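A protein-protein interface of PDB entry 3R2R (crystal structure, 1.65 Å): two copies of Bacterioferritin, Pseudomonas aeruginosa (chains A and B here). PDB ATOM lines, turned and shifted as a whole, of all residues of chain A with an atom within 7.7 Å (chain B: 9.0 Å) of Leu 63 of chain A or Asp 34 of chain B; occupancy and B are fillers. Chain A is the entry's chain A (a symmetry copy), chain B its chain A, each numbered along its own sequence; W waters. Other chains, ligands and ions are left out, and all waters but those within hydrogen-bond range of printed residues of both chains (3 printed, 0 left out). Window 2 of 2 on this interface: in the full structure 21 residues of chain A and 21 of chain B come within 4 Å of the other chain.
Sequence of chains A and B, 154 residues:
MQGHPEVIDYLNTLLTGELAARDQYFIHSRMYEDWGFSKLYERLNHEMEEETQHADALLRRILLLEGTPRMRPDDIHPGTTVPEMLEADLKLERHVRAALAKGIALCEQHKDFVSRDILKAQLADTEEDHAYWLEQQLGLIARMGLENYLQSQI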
ATOM      1  N   MET A   1      17.144   6.001  -7.424  1.00  0.00           N
ATOM      2  CA  MET A   1      17.495   5.252  -6.165  1.00  0.00           C
ATOM      3  C   MET A   1      16.786   5.922  -4.971  1.00  0.00           C
ATOM      4  O   MET A   1      16.919   7.107  -4.782  1.00  0.00           O
ATOM      5  CB  MET A   1      19.017   5.268  -5.959  1.00  0.00           C
ATOM      6  CG  MET A   1      19.453   4.867  -4.567  1.00  0.00           C
ATOM      7  SD  MET A   1      21.238   4.996  -4.233  1.00  0.00           S
ATOM      8  CE  MET A   1      21.550   6.751  -4.411  1.00  0.00           C
ATOM      9  N   ILE A   8      15.984  12.974   2.893  1.00  0.00           N
ATOM     10  CA  ILE A   8      15.364  13.790   1.852  1.00  0.00           C
ATOM     11  C   ILE A   8      14.676  15.005   2.457  1.00  0.00           C
ATOM     12  O   ILE A   8      14.790  16.141   1.957  1.00  0.00           O
ATOM     13  CB  ILE A   8      14.338  12.971   1.009  1.00  0.00           C
ATOM     14  CG1 ILE A   8      15.073  11.848   0.244  1.00  0.00           C
ATOM     15  CG2 ILE A   8      13.576  13.879   0.042  1.00  0.00           C
ATOM     16  CD1 ILE A   8      14.142  10.812  -0.376  1.00  0.00           C
ATOM     17  N   LEU A  11      17.350  17.463   3.525  1.00  0.00           N
ATOM     18  CA  LEU A  11      17.936  18.147   2.351  1.00  0.00           C
ATOM     19  C   LEU A  11      17.011  19.240   1.853  1.00  0.00           C
ATOM     20  O   LEU A  11      17.493  20.287   1.400  1.00  0.00           O
ATOM     21  CB  LEU A  11      18.288  17.161   1.210  1.00  0.00           C
ATOM     22  CG  LEU A  11      19.393  16.170   1.604  1.00  0.00           C
ATOM     23  CD1 LEU A  11      19.640  15.209   0.434  1.00  0.00           C
ATOM     24  CD2 LEU A  11      20.703  16.863   1.972  1.00  0.00           C
ATOM     25  N   ASN A  12      15.688  18.986   1.879  1.00  0.00           N
ATOM     26  CA  ASN A  12      14.709  20.001   1.493  1.00  0.00           C
ATOM     27  C   ASN A  12      14.751  21.214   2.421  1.00  0.00           C
ATOM     28  O   ASN A  12      14.647  22.355   1.971  1.00  0.00           O
ATOM     29  CB  ASN A  12      13.309  19.373   1.419  1.00  0.00           C
ATOM     30  CG  ASN A  12      12.923  18.964   0.036  1.00  0.00           C
ATOM     31  OD1 ASN A  12      13.325  19.598  -0.945  1.00  0.00           O
ATOM     32  ND2 ASN A  12      12.106  17.896  -0.077  1.00  0.00           N
ATOM     33  N   ASP A  56      21.549  24.352  -6.155  1.00  0.00           N
ATOM     34  CA  ASP A  56      21.457  23.450  -7.282  1.00  0.00           C
ATOM     35  C   ASP A  56      21.937  22.062  -6.850  1.00  0.00           C
ATOM     36  O   ASP A  56      21.318  21.047  -7.155  1.00  0.00           O
ATOM     37  CB  ASP A  56      22.330  24.014  -8.419  1.00  0.00           C
ATOM     38  CG  ASP A  56      22.085  23.358  -9.757  1.00  0.00           C
ATOM     39  OD1 ASP A  56      21.099  22.618  -9.966  1.00  0.00           O
ATOM     40  OD2 ASP A  56      22.924  23.605 -10.673  1.00  0.00           O
ATOM     41  N   ALA A  57      23.049  22.016  -6.116  1.00  0.00           N
ATOM     42  CA  ALA A  57      23.598  20.720  -5.654  1.00  0.00           C
ATOM     43  C   ALA A  57      22.569  19.978  -4.799  1.00  0.00           C
ATOM     44  O   ALA A  57      22.401  18.761  -4.937  1.00  0.00           O
ATOM     45  CB  ALA A  57      24.857  20.947  -4.844  1.00  0.00           C
ATOM     46  N   LEU A  58      21.893  20.701  -3.905  1.00  0.00           N
ATOM     47  CA  LEU A  58      20.893  20.052  -3.036  1.00  0.00           C
ATOM     48  C   LEU A  58      19.688  19.599  -3.867  1.00  0.00           C
ATOM     49  O   LEU A  58      19.185  18.477  -3.704  1.00  0.00           O
ATOM     50  CB  LEU A  58      20.413  21.016  -1.936  1.00  0.00           C
ATOM     51  CG  LEU A  58      21.517  21.381  -0.922  1.00  0.00           C
ATOM     52  CD1 LEU A  58      21.103  22.515   0.005  1.00  0.00           C
ATOM     53  CD2 LEU A  58      21.914  20.172  -0.064  1.00  0.00           C
ATOM     54  N   LEU A  59      19.219  20.476  -4.744  1.00  0.00           N
ATOM     55  CA  LEU A  59      18.051  20.164  -5.577  1.00  0.00           C
ATOM     56  C   LEU A  59      18.337  18.905  -6.395  1.00  0.00           C
ATOM     57  O   LEU A  59      17.524  17.981  -6.438  1.00  0.00           O
ATOM     58  CB  LEU A  59      17.796  21.368  -6.495  1.00  0.00           C
ATOM     59  CG  LEU A  59      16.499  21.410  -7.306  1.00  0.00           C
ATOM     60  CD1 LEU A  59      16.520  22.745  -8.073  1.00  0.00           C
ATOM     61  CD2 LEU A  59      16.385  20.299  -8.274  1.00  0.00           C
ATOM     62  N   ARG A  60      19.502  18.857  -7.053  1.00  0.00           N
ATOM     63  CA  ARG A  60      19.818  17.695  -7.873  1.00  0.00           C
ATOM     64  C   ARG A  60      19.918  16.416  -7.033  1.00  0.00           C
ATOM     65  O   ARG A  60      19.522  15.332  -7.491  1.00  0.00           O
ATOM     66  CB  ARG A  60      21.113  17.923  -8.642  1.00  0.00           C
ATOM     67  CG  ARG A  60      20.966  19.028  -9.678  1.00  0.00           C
ATOM     68  CD  ARG A  60      22.252  19.089 -10.513  1.00  0.00           C
ATOM     69  NE  ARG A  60      22.324  20.339 -11.276  1.00  0.00           N
ATOM     70  CZ  ARG A  60      22.534  20.436 -12.584  1.00  0.00           C
ATOM     71  NH1 ARG A  60      22.690  19.353 -13.331  1.00  0.00           N
ATOM     72  NH2 ARG A  60      22.613  21.647 -13.132  1.00  0.00           N
ATOM     73  N   ARG A  61      20.470  16.531  -5.823  1.00  0.00           N
ATOM     74  CA  ARG A  61      20.631  15.346  -4.956  1.00  0.00           C
ATOM     75  C   ARG A  61      19.266  14.843  -4.527  1.00  0.00           C
ATOM     76  O   ARG A  61      19.014  13.641  -4.523  1.00  0.00           O
ATOM     77  CB  ARG A  61      21.519  15.685  -3.756  1.00  0.00           C
ATOM     78  CG  ARG A  61      21.765  14.515  -2.781  1.00  0.00           C
ATOM     79  CD  ARG A  61      22.515  13.344  -3.466  1.00  0.00           C
ATOM     80  NE  ARG A  61      22.768  12.308  -2.454  1.00  0.00           N
ATOM     81  CZ  ARG A  61      23.228  11.105  -2.761  1.00  0.00           C
ATOM     82  NH1 ARG A  61      23.580  10.830  -4.024  1.00  0.00           N
ATOM     83  NH2 ARG A  61      23.347  10.174  -1.797  1.00  0.00           N
ATOM     84  N   ILE A  62      18.367  15.766  -4.191  1.00  0.00           N
ATOM     85  CA  ILE A  62      16.989  15.380  -3.812  1.00  0.00           C
ATOM     86  C   ILE A  62      16.296  14.661  -4.944  1.00  0.00           C
ATOM     87  O   ILE A  62      15.703  13.600  -4.733  1.00  0.00           O
ATOM     88  CB  ILE A  62      16.183  16.621  -3.391  1.00  0.00           C
ATOM     89  CG1 ILE A  62      16.758  17.146  -2.066  1.00  0.00           C
ATOM     90  CG2 ILE A  62      14.647  16.278  -3.227  1.00  0.00           C
ATOM     91  CD1 ILE A  62      16.425  18.633  -1.745  1.00  0.00           C
ATOM     92  N   LEU A  63      16.409  15.177  -6.172  1.00  0.00           N
ATOM     93  CA  LEU A  63      15.820  14.467  -7.303  1.00  0.00           C
ATOM     94  C   LEU A  63      16.456  13.086  -7.507  1.00  0.00           C
ATOM     95  O   LEU A  63      15.749  12.115  -7.822  1.00  0.00           O
ATOM     96  CB  LEU A  63      15.982  15.264  -8.598  1.00  0.00           C
ATOM     97  CG  LEU A  63      15.127  16.525  -8.666  1.00  0.00           C
ATOM     98  CD1 LEU A  63      15.521  17.428  -9.874  1.00  0.00           C
ATOM     99  CD2 LEU A  63      13.619  16.182  -8.718  1.00  0.00           C
ATOM    100  N   LEU A  64      17.782  12.993  -7.403  1.00  0.00           N
ATOM    101  CA  LEU A  64      18.451  11.703  -7.621  1.00  0.00           C
ATOM    102  C   LEU A  64      17.936  10.653  -6.616  1.00  0.00           C
ATOM    103  O   LEU A  64      17.767   9.472  -6.949  1.00  0.00           O
ATOM    104  CB  LEU A  64      19.954  11.915  -7.490  1.00  0.00           C
ATOM    105  CG  LEU A  64      20.844  10.695  -7.716  1.00  0.00           C
ATOM    106  CD1 LEU A  64      22.221  11.177  -8.103  1.00  0.00           C
ATOM    107  CD2 LEU A  64      20.914   9.883  -6.449  1.00  0.00           C
ATOM    108  N   LEU A  65      17.619  11.122  -5.414  1.00  0.00           N
ATOM    109  CA  LEU A  65      17.102  10.271  -4.328  1.00  0.00           C
ATOM    110  C   LEU A  65      15.587  10.059  -4.419  1.00  0.00           C
ATOM    111  O   LEU A  65      14.998   9.481  -3.491  1.00  0.00           O
ATOM    112  CB  LEU A  65      17.456  10.886  -2.965  1.00  0.00           C
ATOM    113  CG  LEU A  65      18.951  10.940  -2.624  1.00  0.00           C
ATOM    114  CD1 LEU A  65      19.233  11.614  -1.316  1.00  0.00           C
ATOM    115  CD2 LEU A  65      19.536   9.547  -2.621  1.00  0.00           C
ATOM    116  N   GLU A  66      14.988  10.477  -5.544  1.00  0.00           N
ATOM    117  CA  GLU A  66      13.561  10.300  -5.829  1.00  0.00           C
ATOM    118  C   GLU A  66      12.652  11.078  -4.861  1.00  0.00           C
ATOM    119  O   GLU A  66      11.496  10.709  -4.650  1.00  0.00           O
ATOM    120  CB  GLU A  66      13.200   8.799  -5.895  1.00  0.00           C
ATOM    121  CG  GLU A  66      14.081   8.048  -6.912  1.00  0.00           C
ATOM    122  CD  GLU A  66      13.701   6.578  -7.136  1.00  0.00           C
ATOM    123  OE1 GLU A  66      12.507   6.245  -7.034  1.00  0.00           O
ATOM    124  OE2 GLU A  66      14.606   5.754  -7.421  1.00  0.00           O
ATOM    125  N   GLY A  67      13.181  12.158  -4.298  1.00  0.00           N
ATOM    126  CA  GLY A  67      12.389  13.116  -3.535  1.00  0.00           C
ATOM    127  C   GLY A  67      11.802  14.230  -4.403  1.00  0.00           C
ATOM    128  O   GLY A  67      12.143  14.377  -5.595  1.00  0.00           O
ATOM    129  N   THR A  68      10.893  15.012  -3.809  1.00  0.00           N
ATOM    130  CA  THR A  68      10.271  16.142  -4.502  1.00  0.00           C
ATOM    131  C   THR A  68      10.847  17.415  -3.869  1.00  0.00           C
ATOM    132  O   THR A  68      10.618  17.666  -2.675  1.00  0.00           O
ATOM    133  CB  THR A  68       8.737  16.094  -4.339  1.00  0.00           C
ATOM    134  OG1 THR A  68       8.238  14.847  -4.871  1.00  0.00           O
ATOM    135  CG2 THR A  68       8.076  17.277  -5.062  1.00  0.00           C
ATOM    136  N   PRO A  69      11.623  18.212  -4.636  1.00  0.00           N
ATOM    137  CA  PRO A  69      12.212  19.399  -3.990  1.00  0.00           C
ATOM    138  C   PRO A  69      11.183  20.448  -3.518  1.00  0.00           C
ATOM    139  O   PRO A  69      10.173  20.674  -4.174  1.00  0.00           O
ATOM    140  CB  PRO A  69      13.101  20.000  -5.084  1.00  0.00           C
ATOM    141  CG  PRO A  69      13.480  18.759  -5.955  1.00  0.00           C
ATOM    142  CD  PRO A  69      12.219  17.943  -5.974  1.00  0.00           C
ATOM    143  N   PHE B  26      13.995  26.700 -12.626  1.00  0.00           N
ATOM    144  CA  PHE B  26      15.048  26.005 -11.868  1.00  0.00           C
ATOM    145  C   PHE B  26      14.623  24.538 -11.604  1.00  0.00           C
ATOM    146  O   PHE B  26      15.323  23.590 -11.973  1.00  0.00           O
ATOM    147  CB  PHE B  26      15.259  26.778 -10.546  1.00  0.00           C
ATOM    148  CG  PHE B  26      16.558  26.511  -9.840  1.00  0.00           C
ATOM    149  CD1 PHE B  26      17.522  25.614 -10.315  1.00  0.00           C
ATOM    150  CD2 PHE B  26      16.816  27.197  -8.635  1.00  0.00           C
ATOM    151  CE1 PHE B  26      18.739  25.423  -9.577  1.00  0.00           C
ATOM    152  CE2 PHE B  26      18.020  27.029  -7.922  1.00  0.00           C
ATOM    153  CZ  PHE B  26      18.983  26.128  -8.390  1.00  0.00           C
ATOM    154  N   ILE B  27      13.462  24.337 -10.975  1.00  0.00           N
ATOM    155  CA  ILE B  27      13.027  22.960 -10.723  1.00  0.00           C
ATOM    156  C   ILE B  27      12.745  22.192 -12.038  1.00  0.00           C
ATOM    157  O   ILE B  27      13.189  21.059 -12.194  1.00  0.00           O
ATOM    158  CB  ILE B  27      11.823  22.872  -9.724  1.00  0.00           C
ATOM    159  CG1 ILE B  27      11.460  21.414  -9.481  1.00  0.00           C
ATOM    160  CG2 ILE B  27      10.611  23.607 -10.222  1.00  0.00           C
ATOM    161  CD1 ILE B  27      12.577  20.612  -8.936  1.00  0.00           C
ATOM    162  N   HIS B  28      12.051  22.788 -12.992  1.00  0.00           N
ATOM    163  CA  HIS B  28      11.750  22.032 -14.216  1.00  0.00           C
ATOM    164  C   HIS B  28      13.027  21.633 -14.971  1.00  0.00           C
ATOM    165  O   HIS B  28      13.130  20.509 -15.442  1.00  0.00           O
ATOM    166  CB  HIS B  28      10.820  22.805 -15.138  1.00  0.00           C
ATOM    167  CG  HIS B  28       9.380  22.732 -14.723  1.00  0.00           C
ATOM    168  ND1 HIS B  28       8.398  23.510 -15.310  1.00  0.00           N
ATOM    169  CD2 HIS B  28       8.745  21.940 -13.818  1.00  0.00           C
ATOM    170  CE1 HIS B  28       7.228  23.226 -14.755  1.00  0.00           C
ATOM    171  NE2 HIS B  28       7.408  22.269 -13.858  1.00  0.00           N
ATOM    172  N   SER B  29      13.989  22.548 -15.094  1.00  0.00           N
ATOM    173  CA  SER B  29      15.206  22.226 -15.865  1.00  0.00           C
ATOM    174  C   SER B  29      15.930  21.069 -15.202  1.00  0.00           C
ATOM    175  O   SER B  29      16.395  20.147 -15.888  1.00  0.00           O
ATOM    176  CB  SER B  29      16.119  23.430 -15.975  1.00  0.00           C
ATOM    177  OG  SER B  29      16.534  23.901 -14.709  1.00  0.00           O
ATOM    178  N   ARG B  30      15.979  21.070 -13.872  1.00  0.00           N
ATOM    179  CA  ARG B  30      16.684  19.970 -13.184  1.00  0.00           C
ATOM    180  C   ARG B  30      15.901  18.664 -13.243  1.00  0.00           C
ATOM    181  O   ARG B  30      16.515  17.604 -13.258  1.00  0.00           O
ATOM    182  CB  ARG B  30      17.086  20.340 -11.746  1.00  0.00           C
ATOM    183  CG  ARG B  30      18.441  21.106 -11.693  1.00  0.00           C
ATOM    184  CD  ARG B  30      18.418  22.397 -12.513  1.00  0.00           C
ATOM    185  NE  ARG B  30      19.662  23.157 -12.299  1.00  0.00           N
ATOM    186  CZ  ARG B  30      20.033  24.212 -13.023  1.00  0.00           C
ATOM    187  NH1 ARG B  30      19.256  24.647 -14.004  1.00  0.00           N
ATOM    188  NH2 ARG B  30      21.184  24.848 -12.739  1.00  0.00           N
ATOM    189  N   MET B  31      14.561  18.729 -13.289  1.00  0.00           N
ATOM    190  CA  MET B  31      13.773  17.521 -13.452  1.00  0.00           C
ATOM    191  C   MET B  31      14.026  16.918 -14.838  1.00  0.00           C
ATOM    192  O   MET B  31      14.172  15.703 -14.977  1.00  0.00           O
ATOM    193  CB  MET B  31      12.278  17.831 -13.293  1.00  0.00           C
ATOM    194  CG  MET B  31      11.916  18.043 -11.826  1.00  0.00           C
ATOM    195  SD  MET B  31      10.201  18.657 -11.689  1.00  0.00           S
ATOM    196  CE  MET B  31       9.271  17.207 -12.263  1.00  0.00           C
ATOM    197  N   TYR B  32      14.089  17.769 -15.851  1.00  0.00           N
ATOM    198  CA  TYR B  32      14.332  17.286 -17.217  1.00  0.00           C
ATOM    199  C   TYR B  32      15.700  16.616 -17.271  1.00  0.00           C
ATOM    200  O   TYR B  32      15.853  15.549 -17.857  1.00  0.00           O
ATOM    201  CB  TYR B  32      14.301  18.448 -18.211  1.00  0.00           C
ATOM    202  CG  TYR B  32      12.921  18.992 -18.515  1.00  0.00           C
ATOM    203  CD1 TYR B  32      11.850  18.135 -18.801  1.00  0.00           C
ATOM    204  CD2 TYR B  32      12.706  20.375 -18.602  1.00  0.00           C
ATOM    205  CE1 TYR B  32      10.574  18.655 -19.154  1.00  0.00           C
ATOM    206  CE2 TYR B  32      11.433  20.897 -18.923  1.00  0.00           C
ATOM    207  CZ  TYR B  32      10.393  20.043 -19.198  1.00  0.00           C
ATOM    208  OH  TYR B  32       9.139  20.556 -19.544  1.00  0.00           O
ATOM    209  N   GLU B  33      16.697  17.259 -16.669  1.00  0.00           N
ATOM    210  CA  GLU B  33      18.054  16.666 -16.583  1.00  0.00           C
ATOM    211  C   GLU B  33      18.036  15.303 -15.883  1.00  0.00           C
ATOM    212  O   GLU B  33      18.651  14.306 -16.341  1.00  0.00           O
ATOM    213  CB  GLU B  33      18.975  17.634 -15.814  1.00  0.00           C
ATOM    214  CG  GLU B  33      20.473  17.231 -15.818  1.00  0.00           C
ATOM    215  CD  GLU B  33      21.139  17.241 -17.201  1.00  0.00           C
ATOM    216  OE1 GLU B  33      22.382  17.187 -17.228  1.00  0.00           O
ATOM    217  OE2 GLU B  33      20.457  17.279 -18.260  1.00  0.00           O
ATOM    218  N   ASP B  34      17.314  15.236 -14.766  1.00  0.00           N
ATOM    219  CA  ASP B  34      17.196  13.988 -13.994  1.00  0.00           C
ATOM    220  C   ASP B  34      16.616  12.843 -14.852  1.00  0.00           C
ATOM    221  O   ASP B  34      16.962  11.680 -14.654  1.00  0.00           O
ATOM    222  CB  ASP B  34      16.327  14.252 -12.753  1.00  0.00           C
ATOM    223  CG  ASP B  34      15.981  12.968 -11.948  1.00  0.00           C
ATOM    224  OD1 ASP B  34      16.886  12.468 -11.284  1.00  0.00           O
ATOM    225  OD2 ASP B  34      14.767  12.589 -11.883  1.00  0.00           O
ATOM    226  N   TRP B  35      15.737  13.165 -15.809  1.00  0.00           N
ATOM    227  CA  TRP B  35      15.146  12.152 -16.646  1.00  0.00           C
ATOM    228  C   TRP B  35      15.949  11.883 -17.929  1.00  0.00           C
ATOM    229  O   TRP B  35      15.608  10.981 -18.681  1.00  0.00           O
ATOM    230  CB  TRP B  35      13.740  12.554 -17.053  1.00  0.00           C
ATOM    231  CG  TRP B  35      12.784  12.595 -15.908  1.00  0.00           C
ATOM    232  CD1 TRP B  35      12.870  11.909 -14.724  1.00  0.00           C
ATOM    233  CD2 TRP B  35      11.580  13.374 -15.838  1.00  0.00           C
ATOM    234  NE1 TRP B  35      11.780  12.217 -13.917  1.00  0.00           N
ATOM    235  CE2 TRP B  35      10.989  13.123 -14.583  1.00  0.00           C
ATOM    236  CE3 TRP B  35      10.958  14.275 -16.718  1.00  0.00           C
ATOM    237  CZ2 TRP B  35       9.795  13.725 -14.191  1.00  0.00           C
ATOM    238  CZ3 TRP B  35       9.749  14.874 -16.325  1.00  0.00           C
ATOM    239  CH2 TRP B  35       9.188  14.595 -15.073  1.00  0.00           C
ATOM    240  N   GLY B  36      16.990  12.650 -18.194  1.00  0.00           N
ATOM    241  CA  GLY B  36      17.838  12.372 -19.365  1.00  0.00           C
ATOM    242  C   GLY B  36      17.485  13.200 -20.597  1.00  0.00           C
ATOM    243  O   GLY B  36      17.949  12.888 -21.715  1.00  0.00           O
ATOM    244  N   PHE B  37      16.709  14.273 -20.420  1.00  0.00           N
ATOM    245  CA  PHE B  37      16.369  15.124 -21.571  1.00  0.00           C
ATOM    246  C   PHE B  37      17.286  16.359 -21.564  1.00  0.00           C
ATOM    247  O   PHE B  37      16.900  17.453 -21.085  1.00  0.00           O
ATOM    248  CB  PHE B  37      14.884  15.528 -21.495  1.00  0.00           C
ATOM    249  CG  PHE B  37      13.948  14.352 -21.568  1.00  0.00           C
ATOM    250  CD1 PHE B  37      13.912  13.548 -22.705  1.00  0.00           C
ATOM    251  CD2 PHE B  37      13.114  14.027 -20.492  1.00  0.00           C
ATOM    252  CE1 PHE B  37      13.081  12.441 -22.778  1.00  0.00           C
ATOM    253  CE2 PHE B  37      12.245  12.918 -20.576  1.00  0.00           C
ATOM    254  CZ  PHE B  37      12.236  12.131 -21.712  1.00  0.00           C
ATOM    255  N   SER B  38      18.506  16.191 -22.077  1.00  0.00           N
ATOM    256  CA  SER B  38      19.489  17.263 -21.985  1.00  0.00           C
ATOM    257  C   SER B  38      19.040  18.510 -22.743  1.00  0.00           C
ATOM    258  O   SER B  38      19.376  19.639 -22.346  1.00  0.00           O
ATOM    259  CB  SER B  38      20.868  16.798 -22.495  1.00  0.00           C
ATOM    260  OG  SER B  38      20.871  16.642 -23.904  1.00  0.00           O
ATOM    261  N   LEU B  40      16.000  19.715 -23.059  1.00  0.00           N
ATOM    262  CA  LEU B  40      15.014  20.461 -22.263  1.00  0.00           C
ATOM    263  C   LEU B  40      15.727  21.103 -21.034  1.00  0.00           C
ATOM    264  O   LEU B  40      15.442  22.246 -20.647  1.00  0.00           O
ATOM    265  CB  LEU B  40      13.849  19.533 -21.853  1.00  0.00           C
ATOM    266  CG  LEU B  40      12.962  19.115 -23.007  1.00  0.00           C
ATOM    267  CD1 LEU B  40      12.022  17.969 -22.592  1.00  0.00           C
ATOM    268  CD2 LEU B  40      12.148  20.328 -23.526  1.00  0.00           C
ATOM    269  N   TYR B  41      16.675  20.384 -20.437  1.00  0.00           N
ATOM    270  CA  TYR B  41      17.495  20.970 -19.372  1.00  0.00           C
ATOM    271  C   TYR B  41      18.160  22.238 -19.873  1.00  0.00           C
ATOM    272  O   TYR B  41      18.124  23.304 -19.206  1.00  0.00           O
ATOM    273  CB  TYR B  41      18.576  19.983 -18.945  1.00  0.00           C
ATOM    274  CG  TYR B  41      19.634  20.677 -18.123  1.00  0.00           C
ATOM    275  CD1 TYR B  41      20.882  20.973 -18.676  1.00  0.00           C
ATOM    276  CD2 TYR B  41      19.374  21.064 -16.816  1.00  0.00           C
ATOM    277  CE1 TYR B  41      21.839  21.616 -17.945  1.00  0.00           C
ATOM    278  CE2 TYR B  41      20.356  21.713 -16.050  1.00  0.00           C
ATOM    279  CZ  TYR B  41      21.573  21.988 -16.631  1.00  0.00           C
ATOM    280  OH  TYR B  41      22.559  22.646 -15.915  1.00  0.00           O
ATOM    281  N   GLY B  79       4.954  20.742 -12.843  1.00  0.00           N
ATOM    282  CA  GLY B  79       4.269  19.537 -13.323  1.00  0.00           C
ATOM    283  C   GLY B  79       4.974  18.277 -12.855  1.00  0.00           C
ATOM    284  O   GLY B  79       6.011  18.347 -12.173  1.00  0.00           O
ATOM    285  N   MET B  85       4.570  19.754 -17.355  1.00  0.00           N
ATOM    286  CA  MET B  85       5.523  20.823 -17.070  1.00  0.00           C
ATOM    287  C   MET B  85       5.461  21.874 -18.176  1.00  0.00           C
ATOM    288  O   MET B  85       5.503  23.065 -17.905  1.00  0.00           O
ATOM    289  CB  MET B  85       6.952  20.267 -16.902  1.00  0.00           C
ATOM    290  CG  MET B  85       7.061  19.229 -15.778  1.00  0.00           C
ATOM    291  SD  MET B  85       8.384  17.978 -15.985  1.00  0.00           S
ATOM    292  CE  MET B  85       9.835  19.018 -15.834  1.00  0.00           C
HETATM  293  O   HOH W   1      13.558  12.109  -9.253  1.00  0.00           O
HETATM  294  O   HOH W   2      15.862  10.224 -10.042  1.00  0.00           O
HETATM  295  O   HOH W   3      24.113  19.288 -15.926  1.00  0.00           O
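Of the 17 printed residues of chain B, 7 touch a printed residue of chain A. Hydrophobic or aromatic side chains of chain B within 4 Å of the printed part of chain A: Phe 26, Ile 27 and Tyr 41. Printed residues of chain A that touch a printed residue of chain B: Asp 56, Leu 59, Arg 60, Leu 63 and Pro 69. Hydrophobic or aromatic side chains of chain A that line the printed part of chain B: Leu 59, Leu 63 and Pro 69. Among the printed residues, 12 pairs touch across the chains.
The backbone carbonyl oxygen (O) of Phe 26 of chain B is in hydrogen-bond range of the side-chain hydroxyl (OG) of Ser 29 of chain B. The side-chain hydroxyl of Ser 29 of chain B lies within hydrogen-bond range of the guanidinium group of Arg 30 of chain B, at 2.9 Å. OD1 of Asp 56 of chain A is in salt-bridge range of NE of Arg 60 of chain A (2.9 Å).
The guanidinium group of Arg 30 of chain B is in salt-bridge range of the side-chain carboxylate of Asp 56 of chain A (2.8 Å). The side-chain hydroxyl of Tyr 41 of chain B sits at hydrogen-bond distance from the guanidinium group of Arg 60 of chain A, 3.0 Å away. NE of Arg 30 of chain B sits close to NH2 of Arg 60 of chain A.
Water W1 bridges the backbone carbonyl oxygen of Leu 63 of chain A (2.6 Å) and the side-chain carboxylate of Asp 34 of chain B (2.9 Å). Water W2 bridges the side-chain carboxylate (OD1) of Asp 34 of chain B (2.8 Å) and the backbone carbonyl oxygen (O) of Leu 63 of chain A (2.9 Å). Water W3 bridges the guanidinium group of Arg 60 of chain A (3.0 Å) and the side-chain carboxylate of Glu 33 of chain B (3.0 Å).
No position is printed for both chains. Of the 12 pairs that touch across the chains among the printed residues, none has its exchanged pair printed and touching as well.
Met 1 of chain A touches none of the printed residues of chain B. Asn 12 of chain A touches none of the printed residues of chain B. Of the printed residues of chain B, Asp 56 of chain A touches Phe 26 (3.7 Å) and Arg 30 (2.8 Å). Of the printed residues of chain B, Arg 60 of chain A touches Arg 30, Glu 33 and Tyr 41. Leu 63 of chain A touches three residues of chain B. Printed residues of chain A within 4 Å of Phe 26 of chain B: Asp 56 and Leu 59. Of the printed residues of chain A, Met 31 of chain B touches Leu 63. Printed residues of chain A within 4 Å of Asp 34 of chain B: Leu 63 (3.7 Å). Printed residues of chain A within 4 Å of Tyr 41 of chain B: Arg 60 (3.0 Å). The nearest printed residue of chain A that does not touch Asp 34 of chain B is Leu 64 of chain A (4.02 Å). The nearest printed residue of chain A that does not touch Ile 27 of chain B is Leu 63 of chain A (4.4 Å).
Among the printed residues, pairs that only touch across the chains: Asp 56 of chain A with Phe 26 of chain B (3.7 Å), Leu 59 of chain A with Phe 26 of chain B (3.8 Å), Leu 59 of chain A with Ile 27 of chain B (3.9 Å), Leu 59 of chain A with Arg 30 of chain B (3.5 Å), Arg 60 of chain A with Glu 33 of chain B (3.95 Å), Leu 63 of chain A with Arg 30 of chain B (3.5 Å), Leu 63 of chain A with Met 31 of chain B (3.8 Å), Leu 63 of chain A with Asp 34 of chain B (3.7 Å) and Pro 69 of chain A with Ile 27 of chain B (3.6 Å).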
